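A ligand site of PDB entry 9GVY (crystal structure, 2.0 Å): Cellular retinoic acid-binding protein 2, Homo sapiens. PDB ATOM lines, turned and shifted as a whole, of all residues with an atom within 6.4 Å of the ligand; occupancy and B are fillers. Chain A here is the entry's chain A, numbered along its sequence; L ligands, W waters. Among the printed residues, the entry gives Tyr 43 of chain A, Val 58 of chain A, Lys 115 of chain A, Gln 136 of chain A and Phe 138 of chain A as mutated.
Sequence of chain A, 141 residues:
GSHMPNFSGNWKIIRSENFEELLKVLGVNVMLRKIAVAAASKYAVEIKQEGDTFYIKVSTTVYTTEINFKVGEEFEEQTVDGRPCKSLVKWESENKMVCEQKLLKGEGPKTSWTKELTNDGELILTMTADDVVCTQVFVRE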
ATOM      1  N   PHE A  19     -33.976 -27.384 -23.556  1.00  0.00           N
ATOM      2  CA  PHE A  19     -33.224 -28.056 -22.498  1.00  0.00           C
ATOM      3  C   PHE A  19     -33.739 -29.474 -22.274  1.00  0.00           C
ATOM      4  O   PHE A  19     -32.969 -30.427 -22.257  1.00  0.00           O
ATOM      5  CB  PHE A  19     -33.164 -27.197 -21.233  1.00  0.00           C
ATOM      6  CG  PHE A  19     -32.233 -27.735 -20.174  1.00  0.00           C
ATOM      7  CD1 PHE A  19     -30.909 -28.061 -20.476  1.00  0.00           C
ATOM      8  CD2 PHE A  19     -32.646 -27.869 -18.855  1.00  0.00           C
ATOM      9  CE1 PHE A  19     -30.032 -28.555 -19.504  1.00  0.00           C
ATOM     10  CE2 PHE A  19     -31.771 -28.363 -17.873  1.00  0.00           C
ATOM     11  CZ  PHE A  19     -30.472 -28.698 -18.199  1.00  0.00           C
ATOM     12  N   LEU A  22     -32.674 -32.007 -24.923  1.00  0.00           N
ATOM     13  CA  LEU A  22     -31.250 -32.347 -24.755  1.00  0.00           C
ATOM     14  C   LEU A  22     -31.097 -33.432 -23.681  1.00  0.00           C
ATOM     15  O   LEU A  22     -30.414 -34.439 -23.871  1.00  0.00           O
ATOM     16  CB  LEU A  22     -30.461 -31.072 -24.388  1.00  0.00           C
ATOM     17  CG  LEU A  22     -28.958 -31.289 -24.102  1.00  0.00           C
ATOM     18  CD1 LEU A  22     -28.167 -31.175 -25.407  1.00  0.00           C
ATOM     19  CD2 LEU A  22     -28.427 -30.242 -23.114  1.00  0.00           C
ATOM     20  N   ALA A  40     -33.085 -25.231 -13.812  1.00  0.00           N
ATOM     21  CA  ALA A  40     -32.328 -24.470 -14.814  1.00  0.00           C
ATOM     22  C   ALA A  40     -32.793 -23.033 -14.829  1.00  0.00           C
ATOM     23  O   ALA A  40     -32.109 -22.164 -15.342  1.00  0.00           O
ATOM     24  CB  ALA A  40     -32.456 -25.069 -16.201  1.00  0.00           C
ATOM     25  N   TYR A  43     -30.200 -20.931 -13.080  1.00  0.00           N
ATOM     26  CA  TYR A  43     -28.771 -20.948 -13.425  1.00  0.00           C
ATOM     27  C   TYR A  43     -28.142 -19.572 -13.269  1.00  0.00           C
ATOM     28  O   TYR A  43     -28.671 -18.595 -13.776  1.00  0.00           O
ATOM     29  CB  TYR A  43     -28.542 -21.374 -14.874  1.00  0.00           C
ATOM     30  CG  TYR A  43     -28.420 -22.855 -15.023  1.00  0.00           C
ATOM     31  CD1 TYR A  43     -27.531 -23.579 -14.241  1.00  0.00           C
ATOM     32  CD2 TYR A  43     -29.137 -23.531 -15.975  1.00  0.00           C
ATOM     33  CE1 TYR A  43     -27.395 -24.949 -14.374  1.00  0.00           C
ATOM     34  CE2 TYR A  43     -29.007 -24.904 -16.139  1.00  0.00           C
ATOM     35  CZ  TYR A  43     -28.151 -25.607 -15.320  1.00  0.00           C
ATOM     36  OH  TYR A  43     -28.081 -26.958 -15.492  1.00  0.00           O
ATOM     37  N   VAL A  45     -24.095 -17.752 -13.581  1.00  0.00           N
ATOM     38  CA  VAL A  45     -22.762 -18.068 -14.093  1.00  0.00           C
ATOM     39  C   VAL A  45     -21.838 -16.927 -13.681  1.00  0.00           C
ATOM     40  O   VAL A  45     -22.188 -15.759 -13.840  1.00  0.00           O
ATOM     41  CB  VAL A  45     -22.793 -18.256 -15.623  1.00  0.00           C
ATOM     42  CG1 VAL A  45     -21.398 -18.487 -16.163  1.00  0.00           C
ATOM     43  CG2 VAL A  45     -23.695 -19.431 -16.034  1.00  0.00           C
ATOM     44  N   ILE A  47     -17.928 -15.623 -14.376  1.00  0.00           N
ATOM     45  CA  ILE A  47     -16.803 -15.834 -15.270  1.00  0.00           C
ATOM     46  C   ILE A  47     -15.731 -14.833 -14.890  1.00  0.00           C
ATOM     47  O   ILE A  47     -16.013 -13.650 -14.776  1.00  0.00           O
ATOM     48  CB  ILE A  47     -17.203 -15.650 -16.758  1.00  0.00           C
ATOM     49  CG1 ILE A  47     -18.315 -16.623 -17.152  1.00  0.00           C
ATOM     50  CG2 ILE A  47     -15.987 -15.799 -17.686  1.00  0.00           C
ATOM     51  CD1 ILE A  47     -18.734 -16.571 -18.639  1.00  0.00           C
ATOM     52  N   ILE A  56     -14.798 -20.428 -14.701  1.00  0.00           N
ATOM     53  CA  ILE A  56     -16.232 -20.334 -14.819  1.00  0.00           C
ATOM     54  C   ILE A  56     -16.860 -21.155 -13.699  1.00  0.00           C
ATOM     55  O   ILE A  56     -16.609 -22.357 -13.575  1.00  0.00           O
ATOM     56  CB  ILE A  56     -16.716 -20.799 -16.203  1.00  0.00           C
ATOM     57  CG1 ILE A  56     -16.053 -20.009 -17.339  1.00  0.00           C
ATOM     58  CG2 ILE A  56     -18.241 -20.746 -16.266  1.00  0.00           C
ATOM     59  CD1 ILE A  56     -16.396 -20.575 -18.727  1.00  0.00           C
ATOM     60  N   VAL A  58     -20.642 -22.250 -12.450  1.00  0.00           N
ATOM     61  CA  VAL A  58     -22.048 -22.360 -12.774  1.00  0.00           C
ATOM     62  C   VAL A  58     -22.790 -22.870 -11.538  1.00  0.00           C
ATOM     63  O   VAL A  58     -22.365 -23.849 -10.915  1.00  0.00           O
ATOM     64  CB  VAL A  58     -22.255 -23.374 -13.926  1.00  0.00           C
ATOM     65  CG1 VAL A  58     -23.721 -23.441 -14.297  1.00  0.00           C
ATOM     66  CG2 VAL A  58     -21.440 -23.040 -15.178  1.00  0.00           C
ATOM     67  N   ILE A  67     -15.067 -24.546 -13.419  1.00  0.00           N
ATOM     68  CA  ILE A  67     -14.090 -25.093 -14.347  1.00  0.00           C
ATOM     69  C   ILE A  67     -13.028 -24.040 -14.605  1.00  0.00           C
ATOM     70  O   ILE A  67     -13.240 -22.832 -14.449  1.00  0.00           O
ATOM     71  CB  ILE A  67     -14.719 -25.607 -15.654  1.00  0.00           C
ATOM     72  CG1 ILE A  67     -15.332 -24.484 -16.481  1.00  0.00           C
ATOM     73  CG2 ILE A  67     -15.718 -26.734 -15.430  1.00  0.00           C
ATOM     74  CD1 ILE A  67     -15.817 -24.960 -17.836  1.00  0.00           C
ATOM     75  N   GLU A  77     -13.791 -32.191 -17.657  1.00  0.00           N
ATOM     76  CA  GLU A  77     -15.019 -31.691 -17.061  1.00  0.00           C
ATOM     77  C   GLU A  77     -16.076 -32.799 -17.179  1.00  0.00           C
ATOM     78  O   GLU A  77     -15.732 -33.963 -17.385  1.00  0.00           O
ATOM     79  CB  GLU A  77     -15.411 -30.354 -17.716  1.00  0.00           C
ATOM     80  CG  GLU A  77     -15.738 -30.409 -19.214  1.00  0.00           C
ATOM     81  CD  GLU A  77     -16.317 -29.124 -19.858  1.00  0.00           C
ATOM     82  OE1 GLU A  77     -16.727 -28.209 -19.115  1.00  0.00           O
ATOM     83  OE2 GLU A  77     -16.366 -29.050 -21.107  1.00  0.00           O
ATOM     84  N   GLN A  78     -17.365 -32.443 -17.094  1.00  0.00           N
ATOM     85  CA  GLN A  78     -18.362 -33.459 -17.381  1.00  0.00           C
ATOM     86  C   GLN A  78     -19.397 -32.956 -18.386  1.00  0.00           C
ATOM     87  O   GLN A  78     -19.639 -31.751 -18.498  1.00  0.00           O
ATOM     88  CB  GLN A  78     -19.033 -33.955 -16.083  1.00  0.00           C
ATOM     89  CG  GLN A  78     -19.616 -32.822 -15.257  1.00  0.00           C
ATOM     90  CD  GLN A  78     -19.343 -32.944 -13.774  1.00  0.00           C
ATOM     91  OE1 GLN A  78     -19.202 -34.051 -13.239  1.00  0.00           O
ATOM     92  NE2 GLN A  78     -19.273 -31.804 -13.104  1.00  0.00           N
ATOM     93  N   THR A  79     -20.003 -33.930 -19.069  1.00  0.00           N
ATOM     94  CA  THR A  79     -21.188 -33.707 -19.874  1.00  0.00           C
ATOM     95  C   THR A  79     -22.307 -33.198 -18.979  1.00  0.00           C
ATOM     96  O   THR A  79     -22.232 -33.284 -17.737  1.00  0.00           O
ATOM     97  CB  THR A  79     -21.631 -35.016 -20.525  1.00  0.00           C
ATOM     98  OG1 THR A  79     -22.120 -35.887 -19.498  1.00  0.00           O
ATOM     99  CG2 THR A  79     -20.512 -35.671 -21.315  1.00  0.00           C
ATOM    100  N   VAL A  80     -23.373 -32.733 -19.645  1.00  0.00           N
ATOM    101  CA  VAL A  80     -24.524 -32.153 -18.965  1.00  0.00           C
ATOM    102  C   VAL A  80     -25.174 -33.174 -18.017  1.00  0.00           C
ATOM    103  O   VAL A  80     -25.681 -32.815 -16.956  1.00  0.00           O
ATOM    104  CB  VAL A  80     -25.531 -31.620 -20.005  1.00  0.00           C
ATOM    105  CG1 VAL A  80     -26.847 -31.234 -19.356  1.00  0.00           C
ATOM    106  CG2 VAL A  80     -24.961 -30.445 -20.786  1.00  0.00           C
ATOM    107  N   ASP A  81     -25.146 -34.458 -18.396  1.00  0.00           N
ATOM    108  CA  ASP A  81     -25.732 -35.533 -17.592  1.00  0.00           C
ATOM    109  C   ASP A  81     -24.685 -36.117 -16.629  1.00  0.00           C
ATOM    110  O   ASP A  81     -24.947 -37.148 -16.009  1.00  0.00           O
ATOM    111  CB  ASP A  81     -26.406 -36.585 -18.481  1.00  0.00           C
ATOM    112  CG  ASP A  81     -25.433 -37.489 -19.231  1.00  0.00           C
ATOM    113  OD1 ASP A  81     -24.565 -36.930 -19.961  1.00  0.00           O
ATOM    114  OD2 ASP A  81     -25.538 -38.727 -19.081  1.00  0.00           O
ATOM    115  N   GLN A 101     -16.104 -32.136 -26.819  1.00  0.00           N
ATOM    116  CA  GLN A 101     -15.928 -33.034 -25.684  1.00  0.00           C
ATOM    117  C   GLN A 101     -15.806 -34.487 -26.156  1.00  0.00           C
ATOM    118  O   GLN A 101     -16.477 -34.895 -27.101  1.00  0.00           O
ATOM    119  CB  GLN A 101     -17.167 -32.925 -24.792  1.00  0.00           C
ATOM    120  CG  GLN A 101     -17.345 -31.531 -24.178  1.00  0.00           C
ATOM    121  CD  GLN A 101     -18.605 -31.419 -23.360  1.00  0.00           C
ATOM    122  OE1 GLN A 101     -19.618 -32.020 -23.695  1.00  0.00           O
ATOM    123  NE2 GLN A 101     -18.546 -30.668 -22.260  1.00  0.00           N
ATOM    124  N   SER A 112     -21.159 -31.045 -27.326  1.00  0.00           N
ATOM    125  CA  SER A 112     -20.265 -29.909 -27.383  1.00  0.00           C
ATOM    126  C   SER A 112     -21.038 -28.717 -26.826  1.00  0.00           C
ATOM    127  O   SER A 112     -22.223 -28.829 -26.530  1.00  0.00           O
ATOM    128  CB  SER A 112     -19.835 -29.654 -28.797  1.00  0.00           C
ATOM    129  OG  SER A 112     -20.973 -29.278 -29.558  1.00  0.00           O
ATOM    130  N   TRP A 113     -20.345 -27.604 -26.650  1.00  0.00           N
ATOM    131  CA  TRP A 113     -20.979 -26.398 -26.193  1.00  0.00           C
ATOM    132  C   TRP A 113     -20.260 -25.223 -26.831  1.00  0.00           C
ATOM    133  O   TRP A 113     -19.099 -25.374 -27.221  1.00  0.00           O
ATOM    134  CB  TRP A 113     -21.006 -26.293 -24.655  1.00  0.00           C
ATOM    135  CG  TRP A 113     -19.691 -26.335 -23.905  1.00  0.00           C
ATOM    136  CD1 TRP A 113     -19.176 -27.398 -23.201  1.00  0.00           C
ATOM    137  CD2 TRP A 113     -18.848 -25.213 -23.616  1.00  0.00           C
ATOM    138  NE1 TRP A 113     -18.019 -27.020 -22.560  1.00  0.00           N
ATOM    139  CE2 TRP A 113     -17.798 -25.681 -22.780  1.00  0.00           C
ATOM    140  CE3 TRP A 113     -18.865 -23.861 -23.982  1.00  0.00           C
ATOM    141  CZ2 TRP A 113     -16.770 -24.853 -22.353  1.00  0.00           C
ATOM    142  CZ3 TRP A 113     -17.832 -23.042 -23.565  1.00  0.00           C
ATOM    143  CH2 TRP A 113     -16.804 -23.528 -22.753  1.00  0.00           C
ATOM    144  N   LYS A 115     -20.062 -20.683 -26.245  1.00  0.00           N
ATOM    145  CA  LYS A 115     -20.448 -19.485 -25.519  1.00  0.00           C
ATOM    146  C   LYS A 115     -20.085 -18.286 -26.391  1.00  0.00           C
ATOM    147  O   LYS A 115     -19.002 -18.265 -26.988  1.00  0.00           O
ATOM    148  CB  LYS A 115     -19.616 -19.336 -24.236  1.00  0.00           C
ATOM    149  CG  LYS A 115     -20.220 -20.000 -22.995  1.00  0.00           C
ATOM    150  CD  LYS A 115     -19.202 -20.095 -21.887  1.00  0.00           C
ATOM    151  CE  LYS A 115     -19.770 -19.901 -20.497  1.00  0.00           C
ATOM    152  NZ  LYS A 115     -20.949 -20.761 -20.249  1.00  0.00           N
ATOM    153  N   LEU A 123     -24.998 -13.054 -22.997  1.00  0.00           N
ATOM    154  CA  LEU A 123     -24.140 -14.212 -23.156  1.00  0.00           C
ATOM    155  C   LEU A 123     -25.009 -15.377 -23.592  1.00  0.00           C
ATOM    156  O   LEU A 123     -26.029 -15.683 -22.986  1.00  0.00           O
ATOM    157  CB  LEU A 123     -23.395 -14.451 -21.840  1.00  0.00           C
ATOM    158  CG  LEU A 123     -22.829 -15.851 -21.668  1.00  0.00           C
ATOM    159  CD1 LEU A 123     -21.587 -16.001 -22.561  1.00  0.00           C
ATOM    160  CD2 LEU A 123     -22.504 -16.092 -20.192  1.00  0.00           C
ATOM    161  N   LEU A 125     -25.236 -19.329 -24.453  1.00  0.00           N
ATOM    162  CA  LEU A 125     -24.658 -20.653 -24.377  1.00  0.00           C
ATOM    163  C   LEU A 125     -25.464 -21.559 -25.289  1.00  0.00           C
ATOM    164  O   LEU A 125     -26.695 -21.522 -25.288  1.00  0.00           O
ATOM    165  CB  LEU A 125     -24.759 -21.165 -22.934  1.00  0.00           C
ATOM    166  CG  LEU A 125     -24.511 -22.673 -22.752  1.00  0.00           C
ATOM    167  CD1 LEU A 125     -23.019 -22.950 -22.804  1.00  0.00           C
ATOM    168  CD2 LEU A 125     -25.058 -23.179 -21.406  1.00  0.00           C
ATOM    169  N   THR A 126     -24.766 -22.389 -26.077  1.00  0.00           N
ATOM    170  CA  THR A 126     -25.466 -23.478 -26.728  1.00  0.00           C
ATOM    171  C   THR A 126     -24.798 -24.767 -26.293  1.00  0.00           C
ATOM    172  O   THR A 126     -23.611 -24.794 -25.976  1.00  0.00           O
ATOM    173  CB  THR A 126     -25.576 -23.313 -28.245  1.00  0.00           C
ATOM    174  OG1 THR A 126     -24.296 -23.771 -28.660  1.00  0.00           O
ATOM    175  CG2 THR A 126     -25.810 -21.888 -28.742  1.00  0.00           C
ATOM    176  N   MET A 127     -25.598 -25.807 -26.158  1.00  0.00           N
ATOM    177  CA  MET A 127     -25.114 -27.105 -25.761  1.00  0.00           C
ATOM    178  C   MET A 127     -25.783 -28.083 -26.706  1.00  0.00           C
ATOM    179  O   MET A 127     -26.979 -27.942 -27.010  1.00  0.00           O
ATOM    180  CB  MET A 127     -25.554 -27.458 -24.342  1.00  0.00           C
ATOM    181  CG  MET A 127     -24.802 -26.695 -23.261  1.00  0.00           C
ATOM    182  SD  MET A 127     -25.506 -26.976 -21.616  1.00  0.00           S
ATOM    183  CE  MET A 127     -27.226 -26.536 -21.814  1.00  0.00           C
ATOM    184  N   GLN A 136     -29.346 -21.212 -24.213  1.00  0.00           N
ATOM    185  CA  GLN A 136     -29.647 -20.539 -22.968  1.00  0.00           C
ATOM    186  C   GLN A 136     -29.046 -19.154 -23.059  1.00  0.00           C
ATOM    187  O   GLN A 136     -27.902 -18.973 -23.510  1.00  0.00           O
ATOM    188  CB  GLN A 136     -29.080 -21.324 -21.781  1.00  0.00           C
ATOM    189  CG  GLN A 136     -29.711 -22.708 -21.643  1.00  0.00           C
ATOM    190  CD  GLN A 136     -29.293 -23.332 -20.330  1.00  0.00           C
ATOM    191  OE1 GLN A 136     -28.222 -23.058 -19.797  1.00  0.00           O
ATOM    192  NE2 GLN A 136     -30.187 -24.113 -19.764  1.00  0.00           N
ATOM    193  N   PHE A 138     -28.175 -15.426 -21.221  1.00  0.00           N
ATOM    194  CA  PHE A 138     -27.941 -14.814 -19.919  1.00  0.00           C
ATOM    195  C   PHE A 138     -27.759 -13.319 -20.098  1.00  0.00           C
ATOM    196  O   PHE A 138     -27.321 -12.878 -21.160  1.00  0.00           O
ATOM    197  CB  PHE A 138     -26.650 -15.340 -19.261  1.00  0.00           C
ATOM    198  CG  PHE A 138     -26.679 -16.814 -18.957  1.00  0.00           C
ATOM    199  CD1 PHE A 138     -26.601 -17.750 -19.983  1.00  0.00           C
ATOM    200  CD2 PHE A 138     -26.808 -17.274 -17.648  1.00  0.00           C
ATOM    201  CE1 PHE A 138     -26.658 -19.118 -19.719  1.00  0.00           C
ATOM    202  CE2 PHE A 138     -26.856 -18.639 -17.383  1.00  0.00           C
ATOM    203  CZ  PHE A 138     -26.749 -19.565 -18.414  1.00  0.00           C
HETATM  204  C1  LIG L   1     -21.485 -26.427 -20.674  1.00  0.00           C
HETATM  205  O1  LIG L   1     -21.638 -25.610 -19.523  1.00  0.00           O
HETATM  206  C2  LIG L   1     -20.903 -24.476 -19.654  1.00  0.00           C
HETATM  207  O2  LIG L   1     -19.775 -24.469 -20.104  1.00  0.00           O
HETATM  208  C3  LIG L   1     -21.553 -23.149 -19.215  1.00  0.00           C
HETATM  209  C4  LIG L   1     -20.759 -21.869 -19.352  1.00  0.00           C
HETATM  210  C5  LIG L   1     -22.952 -22.971 -18.667  1.00  0.00           C
HETATM  211  C6  LIG L   1     -23.770 -24.047 -18.415  1.00  0.00           C
HETATM  212  C7  LIG L   1     -23.172 -25.300 -18.222  1.00  0.00           C
HETATM  213  C8  LIG L   1     -23.955 -26.395 -17.944  1.00  0.00           C
HETATM  214  C9  LIG L   1     -25.321 -26.233 -17.837  1.00  0.00           C
HETATM  215  N1  LIG L   1     -26.051 -27.300 -17.551  1.00  0.00           N
HETATM  216  O3  LIG L   1     -25.484 -28.334 -16.828  1.00  0.00           O
HETATM  217  O4  LIG L   1     -27.270 -27.284 -17.913  1.00  0.00           O
HETATM  218  C10 LIG L   1     -25.920 -24.991 -18.001  1.00  0.00           C
HETATM  219  C11 LIG L   1     -25.132 -23.873 -18.287  1.00  0.00           C
HETATM  220  O   HOH W   1     -20.623 -29.751 -20.197  1.00  0.00           O
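Water W1 lies within hydrogen-bond range of the backbone carbonyl oxygen (O) of Gln 78 (2.8 Å) and the side-chain amide nitrogen (NE2) of Gln 101 (3.1 Å).
NZ of Lys 115 is bonded to C4 of the ligand, at 1.4 Å.
The side-chain hydroxyl (OH) of Tyr 43 lies within hydrogen-bond range of an oxygen (O4) of the ligand (2.6 Å).
Merely in contact with the ligand: Leu 125 (3.2 Å), Phe 19 (3.4 Å), Gln 136 (3.5 Å), Trp 113 (3.5 Å), Val 58 (3.8 Å) and Met 127 (3.9 Å).
Within 4 Å of the ligand: Phe 19, Tyr 43, Val 58, Trp 113, Lys 115, Leu 125, Met 127 and Gln 136.
The nearest printed residue that does not touch the ligand is Val 80 (4.1 Å).
NE1 of Trp 113 is in hydrogen-bond range of OE2 of Glu 77 (3.0 Å).
The backbone NH of Leu 125 is in hydrogen-bond range of the backbone carbonyl oxygen of Gln 136.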
